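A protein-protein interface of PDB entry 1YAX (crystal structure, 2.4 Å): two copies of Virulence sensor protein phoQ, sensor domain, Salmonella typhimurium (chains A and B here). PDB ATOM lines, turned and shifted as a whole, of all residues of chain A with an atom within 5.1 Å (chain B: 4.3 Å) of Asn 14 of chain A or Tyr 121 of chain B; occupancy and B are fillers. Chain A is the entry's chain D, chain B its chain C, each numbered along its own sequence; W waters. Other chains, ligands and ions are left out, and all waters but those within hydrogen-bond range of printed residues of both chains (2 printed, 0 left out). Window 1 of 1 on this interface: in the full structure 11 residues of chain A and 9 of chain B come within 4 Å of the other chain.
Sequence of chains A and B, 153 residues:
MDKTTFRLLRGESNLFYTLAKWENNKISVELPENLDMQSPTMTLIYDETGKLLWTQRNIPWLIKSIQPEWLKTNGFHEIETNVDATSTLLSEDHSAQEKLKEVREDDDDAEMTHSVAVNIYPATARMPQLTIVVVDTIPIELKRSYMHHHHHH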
ATOM      1  N   ARG A  10      10.290   7.198   9.052  1.00  0.00           N
ATOM      2  CA  ARG A  10      10.558   8.341   8.172  1.00  0.00           C
ATOM      3  C   ARG A  10       9.274   8.965   7.644  1.00  0.00           C
ATOM      4  O   ARG A  10       9.165  10.193   7.550  1.00  0.00           O
ATOM      5  CB  ARG A  10      11.448   7.917   6.996  1.00  0.00           C
ATOM      6  CG  ARG A  10      11.673   8.993   5.927  1.00  0.00           C
ATOM      7  CD  ARG A  10      12.423  10.214   6.423  1.00  0.00           C
ATOM      8  NE  ARG A  10      13.847   9.920   6.572  1.00  0.00           N
ATOM      9  CZ  ARG A  10      14.731   9.949   5.581  1.00  0.00           C
ATOM     10  NH1 ARG A  10      16.002   9.664   5.826  1.00  0.00           N
ATOM     11  NH2 ARG A  10      14.365  10.255   4.349  1.00  0.00           N
ATOM     12  N   GLY A  11       8.319   8.127   7.247  1.00  0.00           N
ATOM     13  CA  GLY A  11       7.016   8.620   6.820  1.00  0.00           C
ATOM     14  C   GLY A  11       6.389   9.446   7.929  1.00  0.00           C
ATOM     15  O   GLY A  11       5.873  10.533   7.689  1.00  0.00           O
ATOM     16  N   GLU A  12       6.470   8.921   9.151  1.00  0.00           N
ATOM     17  CA  GLU A  12       5.961   9.602  10.336  1.00  0.00           C
ATOM     18  C   GLU A  12       6.670  10.947  10.578  1.00  0.00           C
ATOM     19  O   GLU A  12       6.016  11.963  10.779  1.00  0.00           O
ATOM     20  CB  GLU A  12       6.116   8.683  11.560  1.00  0.00           C
ATOM     21  CG  GLU A  12       5.400   9.157  12.816  1.00  0.00           C
ATOM     22  CD  GLU A  12       3.894   8.963  12.768  1.00  0.00           C
ATOM     23  OE1 GLU A  12       3.369   8.435  11.757  1.00  0.00           O
ATOM     24  OE2 GLU A  12       3.234   9.343  13.760  1.00  0.00           O
ATOM     25  N   SER A  13       8.003  10.948  10.538  1.00  0.00           N
ATOM     26  CA  SER A  13       8.816  12.154  10.751  1.00  0.00           C
ATOM     27  C   SER A  13       8.500  13.254   9.711  1.00  0.00           C
ATOM     28  O   SER A  13       8.400  14.433  10.055  1.00  0.00           O
ATOM     29  CB  SER A  13      10.316  11.790  10.708  1.00  0.00           C
ATOM     30  OG  SER A  13      11.153  12.938  10.825  1.00  0.00           O
ATOM     31  N   ASN A  14       8.313  12.845   8.460  1.00  0.00           N
ATOM     32  CA  ASN A  14       7.901  13.746   7.383  1.00  0.00           C
ATOM     33  C   ASN A  14       6.509  14.324   7.612  1.00  0.00           C
ATOM     34  O   ASN A  14       6.240  15.478   7.286  1.00  0.00           O
ATOM     35  CB  ASN A  14       7.914  12.993   6.050  1.00  0.00           C
ATOM     36  CG  ASN A  14       9.307  12.820   5.488  1.00  0.00           C
ATOM     37  OD1 ASN A  14      10.263  13.434   5.952  1.00  0.00           O
ATOM     38  ND2 ASN A  14       9.424  11.995   4.467  1.00  0.00           N
ATOM     39  N   LEU A  15       5.627  13.498   8.153  1.00  0.00           N
ATOM     40  CA  LEU A  15       4.234  13.869   8.415  1.00  0.00           C
ATOM     41  C   LEU A  15       4.180  14.977   9.451  1.00  0.00           C
ATOM     42  O   LEU A  15       3.364  15.890   9.350  1.00  0.00           O
ATOM     43  CB  LEU A  15       3.467  12.644   8.932  1.00  0.00           C
ATOM     44  CG  LEU A  15       1.965  12.532   8.718  1.00  0.00           C
ATOM     45  CD1 LEU A  15       1.540  12.965   7.310  1.00  0.00           C
ATOM     46  CD2 LEU A  15       1.551  11.100   9.005  1.00  0.00           C
ATOM     47  N   PHE A  16       5.054  14.881  10.456  1.00  0.00           N
ATOM     48  CA  PHE A  16       5.124  15.904  11.493  1.00  0.00           C
ATOM     49  C   PHE A  16       5.817  17.169  10.972  1.00  0.00           C
ATOM     50  O   PHE A  16       5.529  18.278  11.428  1.00  0.00           O
ATOM     51  CB  PHE A  16       5.793  15.363  12.757  1.00  0.00           C
ATOM     52  CG  PHE A  16       4.826  14.730  13.708  1.00  0.00           C
ATOM     53  CD1 PHE A  16       4.568  13.369  13.652  1.00  0.00           C
ATOM     54  CD2 PHE A  16       4.140  15.508  14.631  1.00  0.00           C
ATOM     55  CE1 PHE A  16       3.656  12.796  14.506  1.00  0.00           C
ATOM     56  CE2 PHE A  16       3.225  14.945  15.487  1.00  0.00           C
ATOM     57  CZ  PHE A  16       2.983  13.585  15.431  1.00  0.00           C
ATOM     58  N   TYR A  17       6.709  17.008  10.000  1.00  0.00           N
ATOM     59  CA  TYR A  17       7.297  18.165   9.347  1.00  0.00           C
ATOM     60  C   TYR A  17       6.220  18.979   8.605  1.00  0.00           C
ATOM     61  O   TYR A  17       6.268  20.198   8.599  1.00  0.00           O
ATOM     62  CB  TYR A  17       8.417  17.765   8.384  1.00  0.00           C
ATOM     63  CG  TYR A  17       9.032  18.976   7.746  1.00  0.00           C
ATOM     64  CD1 TYR A  17       8.721  19.337   6.428  1.00  0.00           C
ATOM     65  CD2 TYR A  17       9.874  19.804   8.480  1.00  0.00           C
ATOM     66  CE1 TYR A  17       9.282  20.484   5.840  1.00  0.00           C
ATOM     67  CE2 TYR A  17      10.430  20.944   7.916  1.00  0.00           C
ATOM     68  CZ  TYR A  17      10.133  21.280   6.592  1.00  0.00           C
ATOM     69  OH  TYR A  17      10.687  22.411   6.045  1.00  0.00           O
ATOM     70  N   THR A  18       5.258  18.300   7.989  1.00  0.00           N
ATOM     71  CA  THR A  18       4.135  18.981   7.344  1.00  0.00           C
ATOM     72  C   THR A  18       3.296  19.714   8.386  1.00  0.00           C
ATOM     73  O   THR A  18       2.868  20.845   8.159  1.00  0.00           O
ATOM     74  CB  THR A  18       3.245  17.986   6.556  1.00  0.00           C
ATOM     75  OG1 THR A  18       3.994  17.401   5.479  1.00  0.00           O
ATOM     76  CG2 THR A  18       2.138  18.716   5.823  1.00  0.00           C
ATOM     77  N   TYR A 121      15.719  18.647   8.643  1.00  0.00           N
ATOM     78  CA  TYR A 121      14.994  19.344   7.581  1.00  0.00           C
ATOM     79  C   TYR A 121      15.598  20.751   7.418  1.00  0.00           C
ATOM     80  O   TYR A 121      15.411  21.607   8.280  1.00  0.00           O
ATOM     81  CB  TYR A 121      13.480  19.386   7.897  1.00  0.00           C
ATOM     82  CG  TYR A 121      12.851  18.007   8.004  1.00  0.00           C
ATOM     83  CD1 TYR A 121      13.043  17.218   9.137  1.00  0.00           C
ATOM     84  CD2 TYR A 121      12.096  17.475   6.970  1.00  0.00           C
ATOM     85  CE1 TYR A 121      12.481  15.941   9.243  1.00  0.00           C
ATOM     86  CE2 TYR A 121      11.526  16.204   7.061  1.00  0.00           C
ATOM     87  CZ  TYR A 121      11.720  15.444   8.203  1.00  0.00           C
ATOM     88  OH  TYR A 121      11.180  14.177   8.330  1.00  0.00           O
ATOM     89  N   SER B  13      12.444  20.876  -1.846  1.00  0.00           N
ATOM     90  CA  SER B  13      11.823  19.566  -1.980  1.00  0.00           C
ATOM     91  C   SER B  13      10.878  19.253  -0.820  1.00  0.00           C
ATOM     92  O   SER B  13       9.782  18.763  -1.012  1.00  0.00           O
ATOM     93  CB  SER B  13      12.884  18.490  -2.085  1.00  0.00           C
ATOM     94  OG  SER B  13      12.283  17.231  -2.232  1.00  0.00           O
ATOM     95  N   ASN B  14      11.314  19.553   0.388  1.00  0.00           N
ATOM     96  CA  ASN B  14      10.500  19.305   1.566  1.00  0.00           C
ATOM     97  C   ASN B  14       9.304  20.218   1.564  1.00  0.00           C
ATOM     98  O   ASN B  14       8.203  19.816   1.906  1.00  0.00           O
ATOM     99  CB  ASN B  14      11.338  19.508   2.836  1.00  0.00           C
ATOM    100  CG  ASN B  14      12.359  18.431   3.015  1.00  0.00           C
ATOM    101  OD1 ASN B  14      12.187  17.311   2.512  1.00  0.00           O
ATOM    102  ND2 ASN B  14      13.432  18.740   3.738  1.00  0.00           N
ATOM    103  N   TYR B  17       6.774  18.945  -0.689  1.00  0.00           N
ATOM    104  CA  TYR B  17       6.135  17.799  -0.068  1.00  0.00           C
ATOM    105  C   TYR B  17       4.984  18.249   0.848  1.00  0.00           C
ATOM    106  O   TYR B  17       3.892  17.679   0.803  1.00  0.00           O
ATOM    107  CB  TYR B  17       7.143  16.947   0.699  1.00  0.00           C
ATOM    108  CG  TYR B  17       6.460  15.905   1.527  1.00  0.00           C
ATOM    109  CD1 TYR B  17       6.320  16.067   2.896  1.00  0.00           C
ATOM    110  CD2 TYR B  17       5.905  14.789   0.931  1.00  0.00           C
ATOM    111  CE1 TYR B  17       5.668  15.114   3.660  1.00  0.00           C
ATOM    112  CE2 TYR B  17       5.256  13.835   1.683  1.00  0.00           C
ATOM    113  CZ  TYR B  17       5.134  14.008   3.047  1.00  0.00           C
ATOM    114  OH  TYR B  17       4.478  13.065   3.795  1.00  0.00           O
ATOM    115  N   ASN B 119      14.726  13.358  -3.680  1.00  0.00           N
ATOM    116  CA  ASN B 119      14.382  12.859  -2.351  1.00  0.00           C
ATOM    117  C   ASN B 119      13.061  12.096  -2.372  1.00  0.00           C
ATOM    118  O   ASN B 119      12.087  12.545  -2.957  1.00  0.00           O
ATOM    119  CB  ASN B 119      14.338  14.007  -1.322  1.00  0.00           C
ATOM    120  CG  ASN B 119      14.608  13.529   0.145  1.00  0.00           C
ATOM    121  OD1 ASN B 119      14.254  14.220   1.105  1.00  0.00           O
ATOM    122  ND2 ASN B 119      15.234  12.352   0.304  1.00  0.00           N
ATOM    123  N   ILE B 120      13.038  10.947  -1.704  1.00  0.00           N
ATOM    124  CA  ILE B 120      11.885  10.058  -1.702  1.00  0.00           C
ATOM    125  C   ILE B 120      11.161  10.210  -0.368  1.00  0.00           C
ATOM    126  O   ILE B 120      11.780  10.195   0.692  1.00  0.00           O
ATOM    127  CB  ILE B 120      12.327   8.587  -1.944  1.00  0.00           C
ATOM    128  CG1 ILE B 120      13.019   8.455  -3.307  1.00  0.00           C
ATOM    129  CG2 ILE B 120      11.126   7.634  -1.881  1.00  0.00           C
ATOM    130  CD1 ILE B 120      13.841   7.203  -3.461  1.00  0.00           C
ATOM    131  N   TYR B 121       9.850  10.390  -0.439  1.00  0.00           N
ATOM    132  CA  TYR B 121       8.999  10.571   0.724  1.00  0.00           C
ATOM    133  C   TYR B 121       8.126   9.324   0.791  1.00  0.00           C
ATOM    134  O   TYR B 121       7.257   9.144  -0.067  1.00  0.00           O
ATOM    135  CB  TYR B 121       8.172  11.861   0.576  1.00  0.00           C
ATOM    136  CG  TYR B 121       9.065  13.080   0.466  1.00  0.00           C
ATOM    137  CD1 TYR B 121       9.597  13.466  -0.762  1.00  0.00           C
ATOM    138  CD2 TYR B 121       9.427  13.809   1.600  1.00  0.00           C
ATOM    139  CE1 TYR B 121      10.447  14.560  -0.865  1.00  0.00           C
ATOM    140  CE2 TYR B 121      10.277  14.891   1.515  1.00  0.00           C
ATOM    141  CZ  TYR B 121      10.791  15.263   0.280  1.00  0.00           C
ATOM    142  OH  TYR B 121      11.649  16.340   0.187  1.00  0.00           O
ATOM    143  N   PRO B 122       8.408   8.433   1.753  1.00  0.00           N
ATOM    144  CA  PRO B 122       7.683   7.160   1.882  1.00  0.00           C
ATOM    145  C   PRO B 122       6.183   7.312   1.979  1.00  0.00           C
ATOM    146  O   PRO B 122       5.718   8.341   2.481  1.00  0.00           O
ATOM    147  CB  PRO B 122       8.226   6.570   3.191  1.00  0.00           C
ATOM    148  CG  PRO B 122       9.552   7.190   3.381  1.00  0.00           C
ATOM    149  CD  PRO B 122       9.477   8.554   2.767  1.00  0.00           C
ATOM    150  N   ALA B 123       5.447   6.302   1.515  1.00  0.00           N
ATOM    151  CA  ALA B 123       3.990   6.337   1.550  1.00  0.00           C
ATOM    152  C   ALA B 123       3.496   6.417   2.989  1.00  0.00           C
ATOM    153  O   ALA B 123       3.999   5.739   3.876  1.00  0.00           O
ATOM    154  CB  ALA B 123       3.391   5.117   0.845  1.00  0.00           C
ATOM    155  N   GLN B 129       3.947   6.925  -2.064  1.00  0.00           N
ATOM    156  CA  GLN B 129       5.353   7.276  -2.173  1.00  0.00           C
ATOM    157  C   GLN B 129       5.575   8.361  -3.233  1.00  0.00           C
ATOM    158  O   GLN B 129       5.149   8.230  -4.384  1.00  0.00           O
ATOM    159  CB  GLN B 129       6.215   6.053  -2.475  1.00  0.00           C
ATOM    160  CG  GLN B 129       7.696   6.322  -2.197  1.00  0.00           C
ATOM    161  CD  GLN B 129       8.611   5.316  -2.834  1.00  0.00           C
ATOM    162  OE1 GLN B 129       8.848   5.368  -4.043  1.00  0.00           O
ATOM    163  NE2 GLN B 129       9.147   4.399  -2.023  1.00  0.00           N
ATOM    164  N   LEU B 130       6.230   9.437  -2.817  1.00  0.00           N
ATOM    165  CA  LEU B 130       6.418  10.615  -3.654  1.00  0.00           C
ATOM    166  C   LEU B 130       7.902  10.799  -3.865  1.00  0.00           C
ATOM    167  O   LEU B 130       8.655  10.864  -2.905  1.00  0.00           O
ATOM    168  CB  LEU B 130       5.824  11.848  -2.971  1.00  0.00           C
ATOM    169  CG  LEU B 130       4.595  12.528  -3.607  1.00  0.00           C
ATOM    170  CD1 LEU B 130       3.682  11.604  -4.437  1.00  0.00           C
ATOM    171  CD2 LEU B 130       3.777  13.269  -2.523  1.00  0.00           C
ATOM    172  N   ILE B 132      10.449  13.448  -5.350  1.00  0.00           N
ATOM    173  CA  ILE B 132      10.541  14.844  -5.774  1.00  0.00           C
ATOM    174  C   ILE B 132      11.946  15.185  -6.270  1.00  0.00           C
ATOM    175  O   ILE B 132      12.946  14.820  -5.665  1.00  0.00           O
ATOM    176  CB  ILE B 132      10.130  15.780  -4.624  1.00  0.00           C
ATOM    177  CG1 ILE B 132       8.712  15.439  -4.164  1.00  0.00           C
ATOM    178  CG2 ILE B 132      10.220  17.247  -5.067  1.00  0.00           C
ATOM    179  CD1 ILE B 132       8.217  16.240  -2.973  1.00  0.00           C
HETATM  180  O   HOH W   1       6.601  10.652   3.909  1.00  0.00           O
HETATM  181  O   HOH W   2      13.314  21.380   5.114  1.00  0.00           O
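Asn 14 of chain A touches Tyr 17 of chain B, and with the chains exchanged Tyr 17 of chain A touches Asn 14 of chain B.
Asn 14 of chain A touches Tyr 121 of chain B, and with the chains exchanged Tyr 121 of chain A touches Asn 14 of chain B.
Positions printed for both chains: 13, 14, 17 and 121.
Of the 10 printed residues of chain A, 5 touch a printed residue of chain B.
Printed residues of chain A that touch a printed residue of chain B: Arg 10, Asn 14, Tyr 17, Thr 18 and Tyr 121.
Along chain A the printed residues that touch a printed residue of chain B span positions 10 to 121.
Of the 11 printed residues of chain B, 4 touch a printed residue of chain A.
Printed residues of chain B that touch a printed residue of chain A: Asn 14, Tyr 17, Tyr 121 and Pro 122.
Hydrophobic or aromatic side chains of chain B within 4 Å of the printed part of chain A: Tyr 17, Tyr 121 and Pro 122.
Among the printed residues, 7 pairs touch across the chains.
Among the printed residues, no Asp or Glu carboxylate lies within 4 Å of a Lys or Arg side-chain nitrogen of the other chain.
Of the printed residues of chain B, Arg 10 of chain A touches Pro 122.
Of chain B, only Tyr 17, Tyr 121 and Pro 122 come within 4 Å of Asn 14 of chain A.
Leu 15 of chain A touches none of the printed residues of chain B.
Phe 16 of chain A touches none of the printed residues of chain B.
Of the printed residues of chain B, Tyr 17 of chain A touches Asn 14 (3.8 Å).
Of the printed residues of chain B, Tyr 121 of chain A touches Asn 14.
Printed residues of chain A within 4 Å of Tyr 17 of chain B: Asn 14 and Thr 18.
Of chain A, only Asn 14 comes within 4 Å of Tyr 121 of chain B.
The nearest printed residue of chain B that does not touch Asn 14 of chain A is Ile 120 of chain B (4.8 Å).
The nearest printed residue of chain A that does not touch Pro 122 of chain B is Gly 11 of chain A (4.2 Å).
OG of Ser 13 of chain B lies within hydrogen-bond range of OH of Tyr 121 of chain B (2.7 Å).
The side-chain amide oxygen (OD1) of Asn 119 of chain B lies within hydrogen-bond range of the side-chain hydroxyl (OH) of Tyr 121 of chain B (3.5 Å).
O of Leu 130 of chain B is in hydrogen-bond range of N of Tyr 121 of chain B (2.8 Å).
OH of Tyr 121 of chain A is in hydrogen-bond range of OG of Ser 13 of chain A (2.8 Å).
The backbone carbonyl oxygen of Asn 14 of chain A is in hydrogen-bond range of the side-chain hydroxyl of Thr 18 of chain A.
The side-chain amide oxygen (OD1) of Asn 14 of chain A is in hydrogen-bond range of the side-chain hydroxyl (OH) of Tyr 121 of chain A (2.7 Å).
Arg 10 of chain A touches Pro 122 of chain B.
CE1 of Tyr 17 of chain B touches O of Asn 14 of chain A, 3.7 Å away.
ND2 of Asn 14 of chain A touches CD2 of Tyr 121 of chain B, 3.4 Å away.
ND2 of Asn 14 of chain A touches CD of Pro 122 of chain B, 3.8 Å away.
Asn 14 of chain B touches Tyr 17 of chain A.
Tyr 17 of chain B touches Thr 18 of chain A (CE1 to OG1, 3.4 Å).
Tyr 121 of chain A touches Asn 14 of chain B (CD2 to ND2, 3.7 Å).
Water W1 lies within hydrogen-bond range of the backbone carbonyl oxygen of Pro 122 of chain B (2.9 Å), the side-chain amide nitrogen of Asn 14 of chain A (3.2 Å) and the side-chain hydroxyl of Tyr 17 of chain B (3.2 Å).
Water W2 bridges the side-chain hydroxyl of Tyr 17 of chain A (3.0 Å) and the side-chain amide nitrogen of Asn 14 of chain B (3.0 Å).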
